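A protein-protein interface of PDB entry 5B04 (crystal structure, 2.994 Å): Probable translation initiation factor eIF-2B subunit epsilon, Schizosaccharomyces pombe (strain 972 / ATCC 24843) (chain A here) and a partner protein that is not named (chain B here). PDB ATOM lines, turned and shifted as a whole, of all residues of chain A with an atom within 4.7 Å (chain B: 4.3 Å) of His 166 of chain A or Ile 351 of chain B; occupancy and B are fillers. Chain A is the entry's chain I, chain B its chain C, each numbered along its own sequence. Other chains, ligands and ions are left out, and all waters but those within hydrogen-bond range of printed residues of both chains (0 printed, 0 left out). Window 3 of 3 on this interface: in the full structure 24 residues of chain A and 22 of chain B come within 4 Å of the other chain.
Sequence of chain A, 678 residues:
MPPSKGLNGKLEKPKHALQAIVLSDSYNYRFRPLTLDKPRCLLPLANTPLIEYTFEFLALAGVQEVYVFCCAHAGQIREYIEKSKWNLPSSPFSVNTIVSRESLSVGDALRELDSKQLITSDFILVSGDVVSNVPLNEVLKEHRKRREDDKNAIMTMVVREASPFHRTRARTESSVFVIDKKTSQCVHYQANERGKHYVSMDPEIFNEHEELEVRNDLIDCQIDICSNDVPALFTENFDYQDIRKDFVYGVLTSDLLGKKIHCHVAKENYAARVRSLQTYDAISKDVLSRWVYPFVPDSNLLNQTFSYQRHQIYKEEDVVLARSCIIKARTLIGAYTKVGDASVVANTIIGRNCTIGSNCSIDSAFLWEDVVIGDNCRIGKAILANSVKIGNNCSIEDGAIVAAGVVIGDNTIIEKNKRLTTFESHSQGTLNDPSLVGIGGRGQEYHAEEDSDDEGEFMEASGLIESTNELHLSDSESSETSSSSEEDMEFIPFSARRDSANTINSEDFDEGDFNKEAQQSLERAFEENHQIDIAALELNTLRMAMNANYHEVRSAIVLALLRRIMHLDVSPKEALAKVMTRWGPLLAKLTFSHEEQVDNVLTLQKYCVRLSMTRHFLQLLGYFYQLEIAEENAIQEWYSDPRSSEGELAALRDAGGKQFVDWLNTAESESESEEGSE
Among the printed residues, merely in contact across the chains: His 166 of chain A with Ile 351 of chain B, Trp 291 of chain A with Ile 351 of chain B, Thr 168 of chain A with Phe 345 of chain B, Trp 291 of chain A with Met 343 of chain B, Trp 291 of chain A with Phe 345 of chain B, His 166 of chain A with Gly 348 of chain B, Arg 167 of chain A with Ser 352 of chain B and Ser 163 of chain A with Gly 348 of chain B.
Pro 164 of chain A touches none of the printed residues of chain B.
Of chain B, only Phe 345, Gly 348 and Ile 351 come within 4 Å of His 166 of chain A.
Of the printed residues of chain B, Thr 168 of chain A touches Phe 345.
Of the printed residues of chain B, Trp 291 of chain A touches Met 343, Phe 345 and Ile 351.
Of the printed residues of chain A, Met 343 of chain B touches Trp 291.
Printed residues of chain A within 4 Å of Phe 345 of chain B: His 166, Thr 168 and Trp 291.
Of chain A, only His 166 and Trp 291 come within 4 Å of Ile 351 of chain B.
The nearest printed residue of chain B that does not touch His 166 of chain A is Glu 347 of chain B (4.8 Å).
The nearest printed residue of chain A that does not touch Ile 351 of chain B is Thr 168 of chain A (6.0 Å).
The nearest printed residue of chain A that does not touch Gly 348 of chain B is Arg 167 of chain A (4.9 Å).
The backbone carbonyl oxygen (O) of Gly 348 of chain B sits at hydrogen-bond distance from the side-chain hydroxyl (OG) of Ser 352 of chain B (2.9 Å).
OG of Ser 352 of chain B lies within hydrogen-bond range of O of Asp 349 of chain B, 2.7 Å away.
OG of Ser 163 of chain A sits close to N of His 166 of chain A (3.4 Å).
N of Thr 168 of chain A sits close to ND1 of His 166 of chain A (3.1 Å).
Of the 12 printed residues of chain B, 5 touch a printed residue of chain A.
Printed residues of chain B that touch a printed residue of chain A: Met 343, Phe 345, Gly 348, Ile 351 and Ser 352.
Hydrophobic or aromatic side chains of chain B within 4 Å of the printed part of chain A: Phe 345 and Ile 351.
Of the 9 printed residues of chain A, 5 touch a printed residue of chain B.
Printed residues of chain A that touch a printed residue of chain B: Ser 163, His 166, Arg 167, Thr 168 and Trp 291.
Among the printed residues, 9 pairs touch across the chains.
Among the printed residues, no Asp or Glu carboxylate lies within 4 Å of a Lys or Arg side-chain nitrogen of the other chain.
NE2 of His 166 of chain A lies within hydrogen-bond range of O of Phe 345 of chain B (2.8 Å).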
ATOM      1  N   ALA A 162      17.058  -6.453  15.806  1.00  0.00           N
ATOM      2  CA  ALA A 162      15.640  -6.584  16.121  1.00  0.00           C
ATOM      3  C   ALA A 162      14.941  -5.228  16.148  1.00  0.00           C
ATOM      4  O   ALA A 162      15.417  -4.259  15.558  1.00  0.00           O
ATOM      5  CB  ALA A 162      15.459  -7.297  17.451  1.00  0.00           C
ATOM      6  N   SER A 163      13.804  -5.174  16.834  1.00  0.00           N
ATOM      7  CA  SER A 163      13.060  -3.934  17.013  1.00  0.00           C
ATOM      8  C   SER A 163      13.133  -3.513  18.481  1.00  0.00           C
ATOM      9  O   SER A 163      13.365  -4.355  19.348  1.00  0.00           O
ATOM     10  CB  SER A 163      11.606  -4.107  16.557  1.00  0.00           C
ATOM     11  OG  SER A 163      10.945  -5.107  17.311  1.00  0.00           O
ATOM     12  N   PRO A 164      12.954  -2.208  18.762  1.00  0.00           N
ATOM     13  CA  PRO A 164      13.021  -1.684  20.133  1.00  0.00           C
ATOM     14  C   PRO A 164      12.158  -2.452  21.128  1.00  0.00           C
ATOM     15  O   PRO A 164      12.628  -2.804  22.210  1.00  0.00           O
ATOM     16  CB  PRO A 164      12.500  -0.254  19.983  1.00  0.00           C
ATOM     17  CG  PRO A 164      12.836   0.118  18.604  1.00  0.00           C
ATOM     18  CD  PRO A 164      12.750  -1.131  17.777  1.00  0.00           C
ATOM     19  N   PHE A 165      10.909  -2.706  20.756  1.00  0.00           N
ATOM     20  CA  PHE A 165       9.962  -3.347  21.657  1.00  0.00           C
ATOM     21  C   PHE A 165       9.729  -4.802  21.273  1.00  0.00           C
ATOM     22  O   PHE A 165       8.652  -5.351  21.512  1.00  0.00           O
ATOM     23  CB  PHE A 165       8.638  -2.583  21.661  1.00  0.00           C
ATOM     24  CG  PHE A 165       8.804  -1.095  21.775  1.00  0.00           C
ATOM     25  CD1 PHE A 165       9.012  -0.499  23.008  1.00  0.00           C
ATOM     26  CD2 PHE A 165       8.757  -0.292  20.647  1.00  0.00           C
ATOM     27  CE1 PHE A 165       9.168   0.870  23.114  1.00  0.00           C
ATOM     28  CE2 PHE A 165       8.913   1.078  20.747  1.00  0.00           C
ATOM     29  CZ  PHE A 165       9.118   1.659  21.981  1.00  0.00           C
ATOM     30  N   HIS A 166      10.742  -5.420  20.674  1.00  0.00           N
ATOM     31  CA  HIS A 166      10.666  -6.823  20.288  1.00  0.00           C
ATOM     32  C   HIS A 166      10.444  -7.690  21.523  1.00  0.00           C
ATOM     33  O   HIS A 166      11.069  -7.475  22.561  1.00  0.00           O
ATOM     34  CB  HIS A 166      11.936  -7.254  19.552  1.00  0.00           C
ATOM     35  CG  HIS A 166      11.763  -8.485  18.719  1.00  0.00           C
ATOM     36  ND1 HIS A 166      11.526  -9.727  19.268  1.00  0.00           N
ATOM     37  CD2 HIS A 166      11.796  -8.666  17.378  1.00  0.00           C
ATOM     38  CE1 HIS A 166      11.417 -10.619  18.301  1.00  0.00           C
ATOM     39  NE2 HIS A 166      11.578 -10.003  17.144  1.00  0.00           N
ATOM     40  N   ARG A 167       9.552  -8.667  21.401  1.00  0.00           N
ATOM     41  CA  ARG A 167       9.143  -9.488  22.536  1.00  0.00           C
ATOM     42  C   ARG A 167      10.288 -10.333  23.088  1.00  0.00           C
ATOM     43  O   ARG A 167      10.237 -10.789  24.231  1.00  0.00           O
ATOM     44  CB  ARG A 167       7.972 -10.386  22.133  1.00  0.00           C
ATOM     45  CG  ARG A 167       6.878  -9.644  21.383  1.00  0.00           C
ATOM     46  CD  ARG A 167       5.495  -9.988  21.905  1.00  0.00           C
ATOM     47  NE  ARG A 167       4.485  -9.066  21.391  1.00  0.00           N
ATOM     48  CZ  ARG A 167       3.175  -9.232  21.534  1.00  0.00           C
ATOM     49  NH1 ARG A 167       2.705 -10.291  22.178  1.00  0.00           N
ATOM     50  NH2 ARG A 167       2.335  -8.338  21.032  1.00  0.00           N
ATOM     51  N   THR A 168      11.318 -10.536  22.275  1.00  0.00           N
ATOM     52  CA  THR A 168      12.492 -11.289  22.700  1.00  0.00           C
ATOM     53  C   THR A 168      13.500 -10.356  23.365  1.00  0.00           C
ATOM     54  O   THR A 168      14.334 -10.786  24.163  1.00  0.00           O
ATOM     55  CB  THR A 168      13.157 -12.014  21.514  1.00  0.00           C
ATOM     56  OG1 THR A 168      12.149 -12.592  20.678  1.00  0.00           O
ATOM     57  CG2 THR A 168      14.093 -13.108  22.007  1.00  0.00           C
ATOM     58  N   ARG A 169      13.408  -9.071  23.035  1.00  0.00           N
ATOM     59  CA  ARG A 169      14.306  -8.064  23.587  1.00  0.00           C
ATOM     60  C   ARG A 169      13.837  -7.605  24.966  1.00  0.00           C
ATOM     61  O   ARG A 169      13.133  -6.603  25.088  1.00  0.00           O
ATOM     62  CB  ARG A 169      14.409  -6.868  22.638  1.00  0.00           C
ATOM     63  CG  ARG A 169      15.520  -5.882  22.971  1.00  0.00           C
ATOM     64  CD  ARG A 169      15.602  -4.785  21.919  1.00  0.00           C
ATOM     65  NE  ARG A 169      16.800  -3.961  22.061  1.00  0.00           N
ATOM     66  CZ  ARG A 169      16.820  -2.757  22.623  1.00  0.00           C
ATOM     67  NH1 ARG A 169      15.704  -2.225  23.099  1.00  0.00           N
ATOM     68  NH2 ARG A 169      17.959  -2.082  22.706  1.00  0.00           N
ATOM     69  N   TRP A 291      11.772 -20.727  14.305  1.00  0.00           N
ATOM     70  CA  TRP A 291      12.842 -19.727  14.269  1.00  0.00           C
ATOM     71  C   TRP A 291      14.242 -20.283  14.526  1.00  0.00           C
ATOM     72  O   TRP A 291      15.225 -19.757  14.004  1.00  0.00           O
ATOM     73  CB  TRP A 291      12.557 -18.613  15.280  1.00  0.00           C
ATOM     74  CG  TRP A 291      11.475 -17.677  14.845  1.00  0.00           C
ATOM     75  CD1 TRP A 291      10.191 -17.639  15.302  1.00  0.00           C
ATOM     76  CD2 TRP A 291      11.579 -16.648  13.852  1.00  0.00           C
ATOM     77  NE1 TRP A 291       9.490 -16.646  14.662  1.00  0.00           N
ATOM     78  CE2 TRP A 291      10.320 -16.024  13.767  1.00  0.00           C
ATOM     79  CE3 TRP A 291      12.615 -16.194  13.031  1.00  0.00           C
ATOM     80  CZ2 TRP A 291      10.068 -14.969  12.892  1.00  0.00           C
ATOM     81  CZ3 TRP A 291      12.364 -15.146  12.164  1.00  0.00           C
ATOM     82  CH2 TRP A 291      11.101 -14.546  12.101  1.00  0.00           C
ATOM     83  N   MET B 343       9.930 -13.918   6.474  1.00  0.00           N
ATOM     84  CA  MET B 343       9.705 -12.698   7.239  1.00  0.00           C
ATOM     85  C   MET B 343      10.910 -12.394   8.120  1.00  0.00           C
ATOM     86  O   MET B 343      11.463 -13.288   8.761  1.00  0.00           O
ATOM     87  CB  MET B 343       8.440 -12.821   8.091  1.00  0.00           C
ATOM     88  CG  MET B 343       8.176 -11.631   9.000  1.00  0.00           C
ATOM     89  SD  MET B 343       7.746 -10.130   8.099  1.00  0.00           S
ATOM     90  CE  MET B 343       6.146 -10.584   7.437  1.00  0.00           C
ATOM     91  N   SER B 344      11.317 -11.130   8.146  1.00  0.00           N
ATOM     92  CA  SER B 344      12.468 -10.720   8.939  1.00  0.00           C
ATOM     93  C   SER B 344      12.145 -10.756  10.428  1.00  0.00           C
ATOM     94  O   SER B 344      11.008 -10.514  10.833  1.00  0.00           O
ATOM     95  CB  SER B 344      12.931  -9.324   8.528  1.00  0.00           C
ATOM     96  OG  SER B 344      14.103  -8.955   9.232  1.00  0.00           O
ATOM     97  N   PHE B 345      13.153 -11.058  11.239  1.00  0.00           N
ATOM     98  CA  PHE B 345      12.959 -11.223  12.674  1.00  0.00           C
ATOM     99  C   PHE B 345      12.788  -9.887  13.392  1.00  0.00           C
ATOM    100  O   PHE B 345      12.158  -9.824  14.447  1.00  0.00           O
ATOM    101  CB  PHE B 345      14.132 -11.995  13.279  1.00  0.00           C
ATOM    102  CG  PHE B 345      13.974 -12.296  14.742  1.00  0.00           C
ATOM    103  CD1 PHE B 345      13.149 -13.326  15.165  1.00  0.00           C
ATOM    104  CD2 PHE B 345      14.656 -11.557  15.693  1.00  0.00           C
ATOM    105  CE1 PHE B 345      13.003 -13.608  16.511  1.00  0.00           C
ATOM    106  CE2 PHE B 345      14.514 -11.833  17.040  1.00  0.00           C
ATOM    107  CZ  PHE B 345      13.687 -12.861  17.449  1.00  0.00           C
ATOM    108  N   GLU B 347      10.968  -7.638  12.544  1.00  0.00           N
ATOM    109  CA  GLU B 347       9.552  -7.300  12.464  1.00  0.00           C
ATOM    110  C   GLU B 347       8.809  -7.914  13.647  1.00  0.00           C
ATOM    111  O   GLU B 347       8.044  -8.865  13.486  1.00  0.00           O
ATOM    112  CB  GLU B 347       8.949  -7.786  11.145  1.00  0.00           C
ATOM    113  CG  GLU B 347       9.295  -6.923   9.944  1.00  0.00           C
ATOM    114  CD  GLU B 347       8.533  -5.612   9.932  1.00  0.00           C
ATOM    115  OE1 GLU B 347       8.965  -4.678   9.222  1.00  0.00           O
ATOM    116  OE2 GLU B 347       7.500  -5.516  10.628  1.00  0.00           O
ATOM    117  N   GLY B 348       9.047  -7.359  14.832  1.00  0.00           N
ATOM    118  CA  GLY B 348       8.514  -7.905  16.068  1.00  0.00           C
ATOM    119  C   GLY B 348       7.002  -8.001  16.130  1.00  0.00           C
ATOM    120  O   GLY B 348       6.458  -9.034  16.519  1.00  0.00           O
ATOM    121  N   ASP B 349       6.321  -6.925  15.752  1.00  0.00           N
ATOM    122  CA  ASP B 349       4.864  -6.886  15.817  1.00  0.00           C
ATOM    123  C   ASP B 349       4.221  -7.884  14.860  1.00  0.00           C
ATOM    124  O   ASP B 349       3.232  -8.531  15.201  1.00  0.00           O
ATOM    125  CB  ASP B 349       4.350  -5.475  15.515  1.00  0.00           C
ATOM    126  CG  ASP B 349       4.681  -4.487  16.616  1.00  0.00           C
ATOM    127  OD1 ASP B 349       4.898  -4.926  17.765  1.00  0.00           O
ATOM    128  OD2 ASP B 349       4.721  -3.272  16.332  1.00  0.00           O
ATOM    129  N   LEU B 350       4.788  -8.008  13.664  1.00  0.00           N
ATOM    130  CA  LEU B 350       4.224  -8.888  12.647  1.00  0.00           C
ATOM    131  C   LEU B 350       4.340 -10.358  13.032  1.00  0.00           C
ATOM    132  O   LEU B 350       3.361 -11.102  12.963  1.00  0.00           O
ATOM    133  CB  LEU B 350       4.902  -8.649  11.296  1.00  0.00           C
ATOM    134  CG  LEU B 350       4.655  -7.287  10.644  1.00  0.00           C
ATOM    135  CD1 LEU B 350       4.995  -7.333   9.162  1.00  0.00           C
ATOM    136  CD2 LEU B 350       3.217  -6.839  10.855  1.00  0.00           C
ATOM    137  N   ILE B 351       5.534 -10.773  13.443  1.00  0.00           N
ATOM    138  CA  ILE B 351       5.779 -12.173  13.773  1.00  0.00           C
ATOM    139  C   ILE B 351       5.038 -12.597  15.039  1.00  0.00           C
ATOM    140  O   ILE B 351       4.799 -13.784  15.260  1.00  0.00           O
ATOM    141  CB  ILE B 351       7.285 -12.455  13.950  1.00  0.00           C
ATOM    142  CG1 ILE B 351       7.837 -11.708  15.167  1.00  0.00           C
ATOM    143  CG2 ILE B 351       8.046 -12.068  12.692  1.00  0.00           C
ATOM    144  CD1 ILE B 351       9.314 -11.935  15.402  1.00  0.00           C
ATOM    145  N   SER B 352       4.668 -11.621  15.863  1.00  0.00           N
ATOM    146  CA  SER B 352       3.946 -11.899  17.097  1.00  0.00           C
ATOM    147  C   SER B 352       2.449 -12.034  16.839  1.00  0.00           C
ATOM    148  O   SER B 352       1.727 -12.647  17.626  1.00  0.00           O
ATOM    149  CB  SER B 352       4.202 -10.796  18.127  1.00  0.00           C
ATOM    150  OG  SER B 352       3.799  -9.532  17.631  1.00  0.00           O
ATOM    151  N   ARG B 353       1.993 -11.464  15.730  1.00  0.00           N
ATOM    152  CA  ARG B 353       0.568 -11.421  15.422  1.00  0.00           C
ATOM    153  C   ARG B 353       0.212 -12.208  14.166  1.00  0.00           C
ATOM    154  O   ARG B 353      -0.903 -12.099  13.657  1.00  0.00           O
ATOM    155  CB  ARG B 353       0.112  -9.970  15.261  1.00  0.00           C
ATOM    156  CG  ARG B 353       0.303  -9.117  16.501  1.00  0.00           C
ATOM    157  CD  ARG B 353       0.164  -7.642  16.168  1.00  0.00           C
ATOM    158  NE  ARG B 353       0.350  -6.795  17.342  1.00  0.00           N
ATOM    159  CZ  ARG B 353       0.503  -5.476  17.293  1.00  0.00           C
ATOM    160  NH1 ARG B 353       0.501  -4.850  16.123  1.00  0.00           N
ATOM    161  NH2 ARG B 353       0.665  -4.783  18.411  1.00  0.00           N
ATOM    162  N   ALA B 354       1.154 -12.999  13.666  1.00  0.00           N
ATOM    163  CA  ALA B 354       0.915 -13.759  12.445  1.00  0.00           C
ATOM    164  C   ALA B 354       1.651 -15.094  12.433  1.00  0.00           C
ATOM    165  O   ALA B 354       2.706 -15.247  13.048  1.00  0.00           O
ATOM    166  CB  ALA B 354       1.309 -12.936  11.229  1.00  0.00           C
ATOM    167  N   ILE B 356       3.839 -17.488  10.382  1.00  0.00           N
ATOM    168  CA  ILE B 356       4.721 -17.465   9.220  1.00  0.00           C
ATOM    169  C   ILE B 356       5.244 -18.864   8.916  1.00  0.00           C
ATOM    170  O   ILE B 356       5.846 -19.512   9.771  1.00  0.00           O
ATOM    171  CB  ILE B 356       5.913 -16.504   9.414  1.00  0.00           C
ATOM    172  CG1 ILE B 356       5.435 -15.049   9.471  1.00  0.00           C
ATOM    173  CG2 ILE B 356       6.898 -16.655   8.272  1.00  0.00           C
ATOM    174  CD1 ILE B 356       5.015 -14.574  10.847  1.00  0.00           C
